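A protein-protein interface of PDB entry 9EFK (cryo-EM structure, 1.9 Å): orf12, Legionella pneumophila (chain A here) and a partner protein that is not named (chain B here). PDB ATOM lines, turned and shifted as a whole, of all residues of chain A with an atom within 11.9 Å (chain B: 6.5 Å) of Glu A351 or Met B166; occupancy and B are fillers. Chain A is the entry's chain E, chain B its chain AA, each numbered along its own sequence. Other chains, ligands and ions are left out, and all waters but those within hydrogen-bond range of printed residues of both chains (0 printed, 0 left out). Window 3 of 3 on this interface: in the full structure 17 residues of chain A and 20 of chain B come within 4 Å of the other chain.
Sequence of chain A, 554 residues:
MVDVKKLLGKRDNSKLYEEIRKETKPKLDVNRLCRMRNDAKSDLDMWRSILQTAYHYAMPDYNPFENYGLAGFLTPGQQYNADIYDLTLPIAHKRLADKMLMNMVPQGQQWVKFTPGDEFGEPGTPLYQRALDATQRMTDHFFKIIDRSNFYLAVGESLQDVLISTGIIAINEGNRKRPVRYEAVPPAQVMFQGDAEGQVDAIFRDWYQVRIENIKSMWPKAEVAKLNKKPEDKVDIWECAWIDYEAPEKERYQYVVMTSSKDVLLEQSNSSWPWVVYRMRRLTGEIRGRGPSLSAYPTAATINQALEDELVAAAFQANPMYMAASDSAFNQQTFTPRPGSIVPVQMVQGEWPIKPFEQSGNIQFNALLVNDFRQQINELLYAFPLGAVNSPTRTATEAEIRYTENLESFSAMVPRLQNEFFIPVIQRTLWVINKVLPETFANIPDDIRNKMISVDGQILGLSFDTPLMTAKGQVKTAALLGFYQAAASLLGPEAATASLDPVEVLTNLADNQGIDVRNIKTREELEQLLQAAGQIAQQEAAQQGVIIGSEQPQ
The side-chain hydroxyl of Ser B169 sits at hydrogen-bond distance from the backbone carbonyl oxygen of Gln A349 (2.9 Å). The side-chain hydroxyl (OG) of Ser B169 is in hydrogen-bond range of the backbone NH (N) of Glu A351 (2.8 Å).
N of Ser A326 sits at hydrogen-bond distance from OE1 of Gln A349, at 3.4 Å.
Among the printed residues, merely in contact across the chains: Gly A350 with Glu B165 (3.6 Å), Gly A350 with Glu B168 (3.7 Å), Gly A350 with Ser B169 (3.3 Å), Glu A351 with Glu B165 (3.6 Å), Glu A351 with Met B166 (3.4 Å) and Trp A352 with Ser B169 (3.6 Å).
Glu A351 touches three residues of chain B. Met B166 touches one residue of chain A. No residue of chain A comes within 4 Å of Gly B163. No residue of chain A comes within 4 Å of Met B164. Of the printed residues of chain A, Glu B168 touches Gly A350. Of the printed residues of chain B, Gly A350 touches Glu B165, Glu B168 and Ser B169. Of the printed residues of chain A, Ser B169 touches Gln A349 (2.9 Å), Gly A350 (3.3 Å), Glu A351 (2.8 Å) and Trp A352 (3.6 Å). Of the printed residues of chain B, Gln A349 touches Ser B169 (2.9 Å). Of the printed residues of chain B, Trp A352 touches Ser B169. Lys A355 touches none of the printed residues of chain B. Gln A346 touches none of the printed residues of chain B. The nearest residue of chain A that does not touch Met B166 is Gly A350 (5.7 Å).
Along chain A the printed residues that touch a printed residue of chain B span positions 349 to 352. Of the 12 printed residues of chain B, 4 touch a printed residue of chain A. Printed residues of chain B that touch a printed residue of chain A: Glu B165, Met B166, Glu B168 and Ser B169.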
ATOM      1  N   MET A 323       2.709 -11.966 -15.542  1.00  0.00           N
ATOM      2  CA  MET A 323       1.411 -12.589 -15.730  1.00  0.00           C
ATOM      3  C   MET A 323       1.580 -14.097 -15.695  1.00  0.00           C
ATOM      4  O   MET A 323       2.554 -14.633 -16.227  1.00  0.00           O
ATOM      5  CB  MET A 323       0.779 -12.178 -17.059  1.00  0.00           C
ATOM      6  CG  MET A 323       0.632 -10.698 -17.248  1.00  0.00           C
ATOM      7  SD  MET A 323      -0.235 -10.276 -18.765  1.00  0.00           S
ATOM      8  CE  MET A 323       0.671 -11.262 -19.940  1.00  0.00           C
ATOM      9  N   ALA A 324       0.635 -14.776 -15.063  1.00  0.00           N
ATOM     10  CA  ALA A 324       0.653 -16.228 -15.009  1.00  0.00           C
ATOM     11  C   ALA A 324      -0.758 -16.703 -14.718  1.00  0.00           C
ATOM     12  O   ALA A 324      -1.660 -15.907 -14.457  1.00  0.00           O
ATOM     13  CB  ALA A 324       1.639 -16.740 -13.956  1.00  0.00           C
ATOM     14  N   ALA A 325      -0.940 -18.020 -14.776  1.00  0.00           N
ATOM     15  CA  ALA A 325      -2.203 -18.599 -14.342  1.00  0.00           C
ATOM     16  C   ALA A 325      -2.448 -18.345 -12.863  1.00  0.00           C
ATOM     17  O   ALA A 325      -3.590 -18.137 -12.450  1.00  0.00           O
ATOM     18  CB  ALA A 325      -2.228 -20.095 -14.643  1.00  0.00           C
ATOM     19  N   SER A 326      -1.395 -18.349 -12.052  1.00  0.00           N
ATOM     20  CA  SER A 326      -1.541 -18.164 -10.618  1.00  0.00           C
ATOM     21  C   SER A 326      -0.306 -17.473 -10.070  1.00  0.00           C
ATOM     22  O   SER A 326       0.794 -17.629 -10.600  1.00  0.00           O
ATOM     23  CB  SER A 326      -1.763 -19.506  -9.910  1.00  0.00           C
ATOM     24  OG  SER A 326      -1.730 -19.359  -8.505  1.00  0.00           O
ATOM     25  N   GLN A 346       7.670 -22.287 -11.493  1.00  0.00           N
ATOM     26  CA  GLN A 346       6.842 -23.084 -12.394  1.00  0.00           C
ATOM     27  C   GLN A 346       6.728 -22.329 -13.707  1.00  0.00           C
ATOM     28  O   GLN A 346       5.887 -21.444 -13.858  1.00  0.00           O
ATOM     29  CB  GLN A 346       5.471 -23.345 -11.784  1.00  0.00           C
ATOM     30  CG  GLN A 346       5.511 -23.982 -10.419  1.00  0.00           C
ATOM     31  CD  GLN A 346       4.136 -24.345  -9.914  1.00  0.00           C
ATOM     32  OE1 GLN A 346       3.430 -25.135 -10.531  1.00  0.00           O
ATOM     33  NE2 GLN A 346       3.744 -23.764  -8.794  1.00  0.00           N
ATOM     34  N   MET A 347       7.592 -22.666 -14.664  1.00  0.00           N
ATOM     35  CA  MET A 347       7.709 -21.860 -15.870  1.00  0.00           C
ATOM     36  C   MET A 347       6.522 -22.025 -16.810  1.00  0.00           C
ATOM     37  O   MET A 347       6.291 -21.150 -17.647  1.00  0.00           O
ATOM     38  CB  MET A 347       9.023 -22.189 -16.578  1.00  0.00           C
ATOM     39  CG  MET A 347      10.230 -21.564 -15.886  1.00  0.00           C
ATOM     40  SD  MET A 347      11.818 -22.278 -16.325  1.00  0.00           S
ATOM     41  CE  MET A 347      11.711 -22.221 -18.104  1.00  0.00           C
ATOM     42  N   VAL A 348       5.774 -23.117 -16.702  1.00  0.00           N
ATOM     43  CA  VAL A 348       4.521 -23.287 -17.431  1.00  0.00           C
ATOM     44  C   VAL A 348       3.479 -23.825 -16.461  1.00  0.00           C
ATOM     45  O   VAL A 348       3.749 -24.774 -15.720  1.00  0.00           O
ATOM     46  CB  VAL A 348       4.671 -24.231 -18.640  1.00  0.00           C
ATOM     47  CG1 VAL A 348       3.333 -24.425 -19.322  1.00  0.00           C
ATOM     48  CG2 VAL A 348       5.684 -23.684 -19.623  1.00  0.00           C
ATOM     49  N   GLN A 349       2.297 -23.216 -16.456  1.00  0.00           N
ATOM     50  CA  GLN A 349       1.177 -23.668 -15.631  1.00  0.00           C
ATOM     51  C   GLN A 349      -0.006 -23.938 -16.552  1.00  0.00           C
ATOM     52  O   GLN A 349      -0.675 -23.006 -17.004  1.00  0.00           O
ATOM     53  CB  GLN A 349       0.832 -22.641 -14.559  1.00  0.00           C
ATOM     54  CG  GLN A 349       1.805 -22.619 -13.403  1.00  0.00           C
ATOM     55  CD  GLN A 349       1.470 -21.569 -12.372  1.00  0.00           C
ATOM     56  OE1 GLN A 349       1.199 -20.419 -12.702  1.00  0.00           O
ATOM     57  NE2 GLN A 349       1.485 -21.961 -11.109  1.00  0.00           N
ATOM     58  N   GLY A 350      -0.268 -25.212 -16.822  1.00  0.00           N
ATOM     59  CA  GLY A 350      -1.300 -25.586 -17.766  1.00  0.00           C
ATOM     60  C   GLY A 350      -0.979 -25.138 -19.175  1.00  0.00           C
ATOM     61  O   GLY A 350       0.055 -25.514 -19.731  1.00  0.00           O
ATOM     62  N   GLU A 351      -1.863 -24.339 -19.767  1.00  0.00           N
ATOM     63  CA  GLU A 351      -1.648 -23.845 -21.119  1.00  0.00           C
ATOM     64  C   GLU A 351      -0.799 -22.584 -21.169  1.00  0.00           C
ATOM     65  O   GLU A 351      -0.335 -22.214 -22.250  1.00  0.00           O
ATOM     66  CB  GLU A 351      -2.992 -23.558 -21.795  1.00  0.00           C
ATOM     67  CG  GLU A 351      -3.893 -24.757 -21.960  1.00  0.00           C
ATOM     68  CD  GLU A 351      -5.222 -24.398 -22.597  1.00  0.00           C
ATOM     69  OE1 GLU A 351      -5.699 -23.264 -22.388  1.00  0.00           O
ATOM     70  OE2 GLU A 351      -5.791 -25.250 -23.310  1.00  0.00           O
ATOM     71  N   TRP A 352      -0.584 -21.918 -20.041  1.00  0.00           N
ATOM     72  CA  TRP A 352      -0.051 -20.570 -20.047  1.00  0.00           C
ATOM     73  C   TRP A 352       1.318 -20.523 -19.385  1.00  0.00           C
ATOM     74  O   TRP A 352       1.475 -21.010 -18.258  1.00  0.00           O
ATOM     75  CB  TRP A 352      -1.012 -19.612 -19.326  1.00  0.00           C
ATOM     76  CG  TRP A 352      -2.394 -19.612 -19.906  1.00  0.00           C
ATOM     77  CD1 TRP A 352      -2.735 -19.854 -21.199  1.00  0.00           C
ATOM     78  CD2 TRP A 352      -3.620 -19.376 -19.206  1.00  0.00           C
ATOM     79  NE1 TRP A 352      -4.094 -19.775 -21.354  1.00  0.00           N
ATOM     80  CE2 TRP A 352      -4.661 -19.484 -20.143  1.00  0.00           C
ATOM     81  CE3 TRP A 352      -3.936 -19.077 -17.881  1.00  0.00           C
ATOM     82  CZ2 TRP A 352      -5.994 -19.305 -19.797  1.00  0.00           C
ATOM     83  CZ3 TRP A 352      -5.260 -18.904 -17.539  1.00  0.00           C
ATOM     84  CH2 TRP A 352      -6.273 -19.019 -18.492  1.00  0.00           C
ATOM     85  N   PRO A 353       2.325 -19.964 -20.043  1.00  0.00           N
ATOM     86  CA  PRO A 353       3.610 -19.721 -19.387  1.00  0.00           C
ATOM     87  C   PRO A 353       3.623 -18.383 -18.662  1.00  0.00           C
ATOM     88  O   PRO A 353       2.850 -17.473 -18.961  1.00  0.00           O
ATOM     89  CB  PRO A 353       4.590 -19.709 -20.564  1.00  0.00           C
ATOM     90  CG  PRO A 353       3.785 -19.153 -21.676  1.00  0.00           C
ATOM     91  CD  PRO A 353       2.374 -19.645 -21.479  1.00  0.00           C
ATOM     92  N   ILE A 354       4.528 -18.275 -17.698  1.00  0.00           N
ATOM     93  CA  ILE A 354       4.723 -17.013 -16.994  1.00  0.00           C
ATOM     94  C   ILE A 354       5.568 -16.094 -17.866  1.00  0.00           C
ATOM     95  O   ILE A 354       6.606 -16.498 -18.399  1.00  0.00           O
ATOM     96  CB  ILE A 354       5.364 -17.243 -15.615  1.00  0.00           C
ATOM     97  CG1 ILE A 354       5.589 -15.909 -14.905  1.00  0.00           C
ATOM     98  CG2 ILE A 354       6.654 -18.036 -15.726  1.00  0.00           C
ATOM     99  CD1 ILE A 354       6.066 -16.047 -13.485  1.00  0.00           C
ATOM    100  N   LYS A 355       5.102 -14.868 -18.051  1.00  0.00           N
ATOM    101  CA  LYS A 355       5.722 -13.910 -18.950  1.00  0.00           C
ATOM    102  C   LYS A 355       5.647 -12.529 -18.324  1.00  0.00           C
ATOM    103  O   LYS A 355       4.849 -12.301 -17.411  1.00  0.00           O
ATOM    104  CB  LYS A 355       5.039 -13.912 -20.324  1.00  0.00           C
ATOM    105  CG  LYS A 355       3.551 -13.675 -20.273  1.00  0.00           C
ATOM    106  CD  LYS A 355       2.977 -13.460 -21.659  1.00  0.00           C
ATOM    107  CE  LYS A 355       3.443 -14.524 -22.631  1.00  0.00           C
ATOM    108  NZ  LYS A 355       3.130 -15.895 -22.161  1.00  0.00           N
ATOM    109  N   TYR B 140     -10.246 -34.767 -15.771  1.00  0.00           N
ATOM    110  CA  TYR B 140      -9.484 -34.884 -17.010  1.00  0.00           C
ATOM    111  C   TYR B 140      -8.103 -35.480 -16.774  1.00  0.00           C
ATOM    112  O   TYR B 140      -7.626 -36.285 -17.579  1.00  0.00           O
ATOM    113  CB  TYR B 140      -9.353 -33.522 -17.682  1.00  0.00           C
ATOM    114  CG  TYR B 140     -10.466 -33.183 -18.639  1.00  0.00           C
ATOM    115  CD1 TYR B 140     -10.472 -33.684 -19.928  1.00  0.00           C
ATOM    116  CD2 TYR B 140     -11.499 -32.342 -18.260  1.00  0.00           C
ATOM    117  CE1 TYR B 140     -11.476 -33.369 -20.806  1.00  0.00           C
ATOM    118  CE2 TYR B 140     -12.510 -32.024 -19.133  1.00  0.00           C
ATOM    119  CZ  TYR B 140     -12.493 -32.539 -20.404  1.00  0.00           C
ATOM    120  OH  TYR B 140     -13.499 -32.222 -21.280  1.00  0.00           O
ATOM    121  N   SER B 161      -5.799 -34.827 -23.041  1.00  0.00           N
ATOM    122  CA  SER B 161      -4.697 -34.106 -22.417  1.00  0.00           C
ATOM    123  C   SER B 161      -4.866 -32.602 -22.561  1.00  0.00           C
ATOM    124  O   SER B 161      -4.508 -31.843 -21.656  1.00  0.00           O
ATOM    125  CB  SER B 161      -3.367 -34.550 -23.020  1.00  0.00           C
ATOM    126  OG  SER B 161      -3.086 -35.890 -22.677  1.00  0.00           O
ATOM    127  N   GLN B 162      -5.388 -32.152 -23.703  1.00  0.00           N
ATOM    128  CA  GLN B 162      -5.657 -30.729 -23.881  1.00  0.00           C
ATOM    129  C   GLN B 162      -6.700 -30.243 -22.889  1.00  0.00           C
ATOM    130  O   GLN B 162      -6.579 -29.145 -22.340  1.00  0.00           O
ATOM    131  CB  GLN B 162      -6.116 -30.452 -25.311  1.00  0.00           C
ATOM    132  CG  GLN B 162      -5.008 -30.510 -26.337  1.00  0.00           C
ATOM    133  CD  GLN B 162      -5.526 -30.453 -27.759  1.00  0.00           C
ATOM    134  OE1 GLN B 162      -6.591 -29.897 -28.025  1.00  0.00           O
ATOM    135  NE2 GLN B 162      -4.778 -31.039 -28.683  1.00  0.00           N
ATOM    136  N   GLY B 163      -7.741 -31.043 -22.657  1.00  0.00           N
ATOM    137  CA  GLY B 163      -8.727 -30.690 -21.655  1.00  0.00           C
ATOM    138  C   GLY B 163      -8.147 -30.617 -20.259  1.00  0.00           C
ATOM    139  O   GLY B 163      -8.568 -29.789 -19.452  1.00  0.00           O
ATOM    140  N   MET B 164      -7.179 -31.481 -19.952  1.00  0.00           N
ATOM    141  CA  MET B 164      -6.514 -31.426 -18.657  1.00  0.00           C
ATOM    142  C   MET B 164      -5.745 -30.124 -18.488  1.00  0.00           C
ATOM    143  O   MET B 164      -5.822 -29.475 -17.441  1.00  0.00           O
ATOM    144  CB  MET B 164      -5.575 -32.617 -18.502  1.00  0.00           C
ATOM    145  CG  MET B 164      -4.741 -32.582 -17.247  1.00  0.00           C
ATOM    146  SD  MET B 164      -3.326 -33.683 -17.348  1.00  0.00           S
ATOM    147  CE  MET B 164      -2.316 -32.819 -18.540  1.00  0.00           C
ATOM    148  N   GLU B 165      -4.989 -29.727 -19.511  1.00  0.00           N
ATOM    149  CA  GLU B 165      -4.192 -28.512 -19.410  1.00  0.00           C
ATOM    150  C   GLU B 165      -5.064 -27.270 -19.413  1.00  0.00           C
ATOM    151  O   GLU B 165      -4.714 -26.270 -18.780  1.00  0.00           O
ATOM    152  CB  GLU B 165      -3.183 -28.452 -20.552  1.00  0.00           C
ATOM    153  CG  GLU B 165      -2.203 -29.597 -20.551  1.00  0.00           C
ATOM    154  CD  GLU B 165      -1.310 -29.592 -21.766  1.00  0.00           C
ATOM    155  OE1 GLU B 165      -1.333 -28.594 -22.516  1.00  0.00           O
ATOM    156  OE2 GLU B 165      -0.588 -30.586 -21.975  1.00  0.00           O
ATOM    157  N   MET B 166      -6.187 -27.309 -20.125  1.00  0.00           N
ATOM    158  CA  MET B 166      -7.077 -26.158 -20.165  1.00  0.00           C
ATOM    159  C   MET B 166      -7.695 -25.897 -18.799  1.00  0.00           C
ATOM    160  O   MET B 166      -7.710 -24.760 -18.322  1.00  0.00           O
ATOM    161  CB  MET B 166      -8.159 -26.375 -21.221  1.00  0.00           C
ATOM    162  CG  MET B 166      -9.047 -25.174 -21.444  1.00  0.00           C
ATOM    163  SD  MET B 166     -10.554 -25.205 -20.469  1.00  0.00           S
ATOM    164  CE  MET B 166     -11.516 -26.398 -21.383  1.00  0.00           C
ATOM    165  N   TRP B 167      -8.203 -26.943 -18.149  1.00  0.00           N
ATOM    166  CA  TRP B 167      -8.824 -26.771 -16.847  1.00  0.00           C
ATOM    167  C   TRP B 167      -7.810 -26.577 -15.735  1.00  0.00           C
ATOM    168  O   TRP B 167      -8.173 -26.070 -14.675  1.00  0.00           O
ATOM    169  CB  TRP B 167      -9.732 -27.955 -16.528  1.00  0.00           C
ATOM    170  CG  TRP B 167     -11.009 -27.876 -17.275  1.00  0.00           C
ATOM    171  CD1 TRP B 167     -11.420 -28.689 -18.281  1.00  0.00           C
ATOM    172  CD2 TRP B 167     -12.034 -26.894 -17.108  1.00  0.00           C
ATOM    173  NE1 TRP B 167     -12.644 -28.287 -18.743  1.00  0.00           N
ATOM    174  CE2 TRP B 167     -13.043 -27.183 -18.039  1.00  0.00           C
ATOM    175  CE3 TRP B 167     -12.196 -25.799 -16.255  1.00  0.00           C
ATOM    176  CZ2 TRP B 167     -14.202 -26.422 -18.141  1.00  0.00           C
ATOM    177  CZ3 TRP B 167     -13.342 -25.046 -16.357  1.00  0.00           C
ATOM    178  CH2 TRP B 167     -14.333 -25.359 -17.292  1.00  0.00           C
ATOM    179  N   GLU B 168      -6.555 -26.967 -15.946  1.00  0.00           N
ATOM    180  CA  GLU B 168      -5.534 -26.664 -14.954  1.00  0.00           C
ATOM    181  C   GLU B 168      -5.289 -25.164 -14.864  1.00  0.00           C
ATOM    182  O   GLU B 168      -5.190 -24.614 -13.765  1.00  0.00           O
ATOM    183  CB  GLU B 168      -4.240 -27.398 -15.280  1.00  0.00           C
ATOM    184  CG  GLU B 168      -3.169 -27.211 -14.229  1.00  0.00           C
ATOM    185  CD  GLU B 168      -1.891 -27.940 -14.559  1.00  0.00           C
ATOM    186  OE1 GLU B 168      -1.802 -28.525 -15.655  1.00  0.00           O
ATOM    187  OE2 GLU B 168      -0.972 -27.927 -13.718  1.00  0.00           O
ATOM    188  N   SER B 169      -5.187 -24.490 -16.009  1.00  0.00           N
ATOM    189  CA  SER B 169      -4.983 -23.046 -16.003  1.00  0.00           C
ATOM    190  C   SER B 169      -6.186 -22.320 -15.424  1.00  0.00           C
ATOM    191  O   SER B 169      -6.031 -21.365 -14.659  1.00  0.00           O
ATOM    192  CB  SER B 169      -4.698 -22.550 -17.414  1.00  0.00           C
ATOM    193  OG  SER B 169      -3.483 -23.078 -17.893  1.00  0.00           O
ATOM    194  N   ARG B 170      -7.392 -22.749 -15.788  1.00  0.00           N
ATOM    195  CA  ARG B 170      -8.588 -22.083 -15.291  1.00  0.00           C
ATOM    196  C   ARG B 170      -8.778 -22.320 -13.799  1.00  0.00           C
ATOM    197  O   ARG B 170      -9.186 -21.409 -13.071  1.00  0.00           O
ATOM    198  CB  ARG B 170      -9.806 -22.547 -16.077  1.00  0.00           C
ATOM    199  CG  ARG B 170      -9.692 -22.264 -17.554  1.00  0.00           C
ATOM    200  CD  ARG B 170     -11.022 -22.413 -18.243  1.00  0.00           C
ATOM    201  NE  ARG B 170     -12.005 -21.490 -17.697  1.00  0.00           N
ATOM    202  CZ  ARG B 170     -13.236 -21.351 -18.163  1.00  0.00           C
ATOM    203  NH1 ARG B 170     -13.664 -22.054 -19.196  1.00  0.00           N
ATOM    204  NH2 ARG B 170     -14.056 -20.485 -17.580  1.00  0.00           N
ATOM    205  N   ALA B 171      -8.494 -23.533 -13.323  1.00  0.00           N
ATOM    206  CA  ALA B 171      -8.573 -23.791 -11.891  1.00  0.00           C
ATOM    207  C   ALA B 171      -7.529 -22.988 -11.127  1.00  0.00           C
ATOM    208  O   ALA B 171      -7.819 -22.454 -10.054  1.00  0.00           O
ATOM    209  CB  ALA B 171      -8.409 -25.281 -11.609  1.00  0.00           C
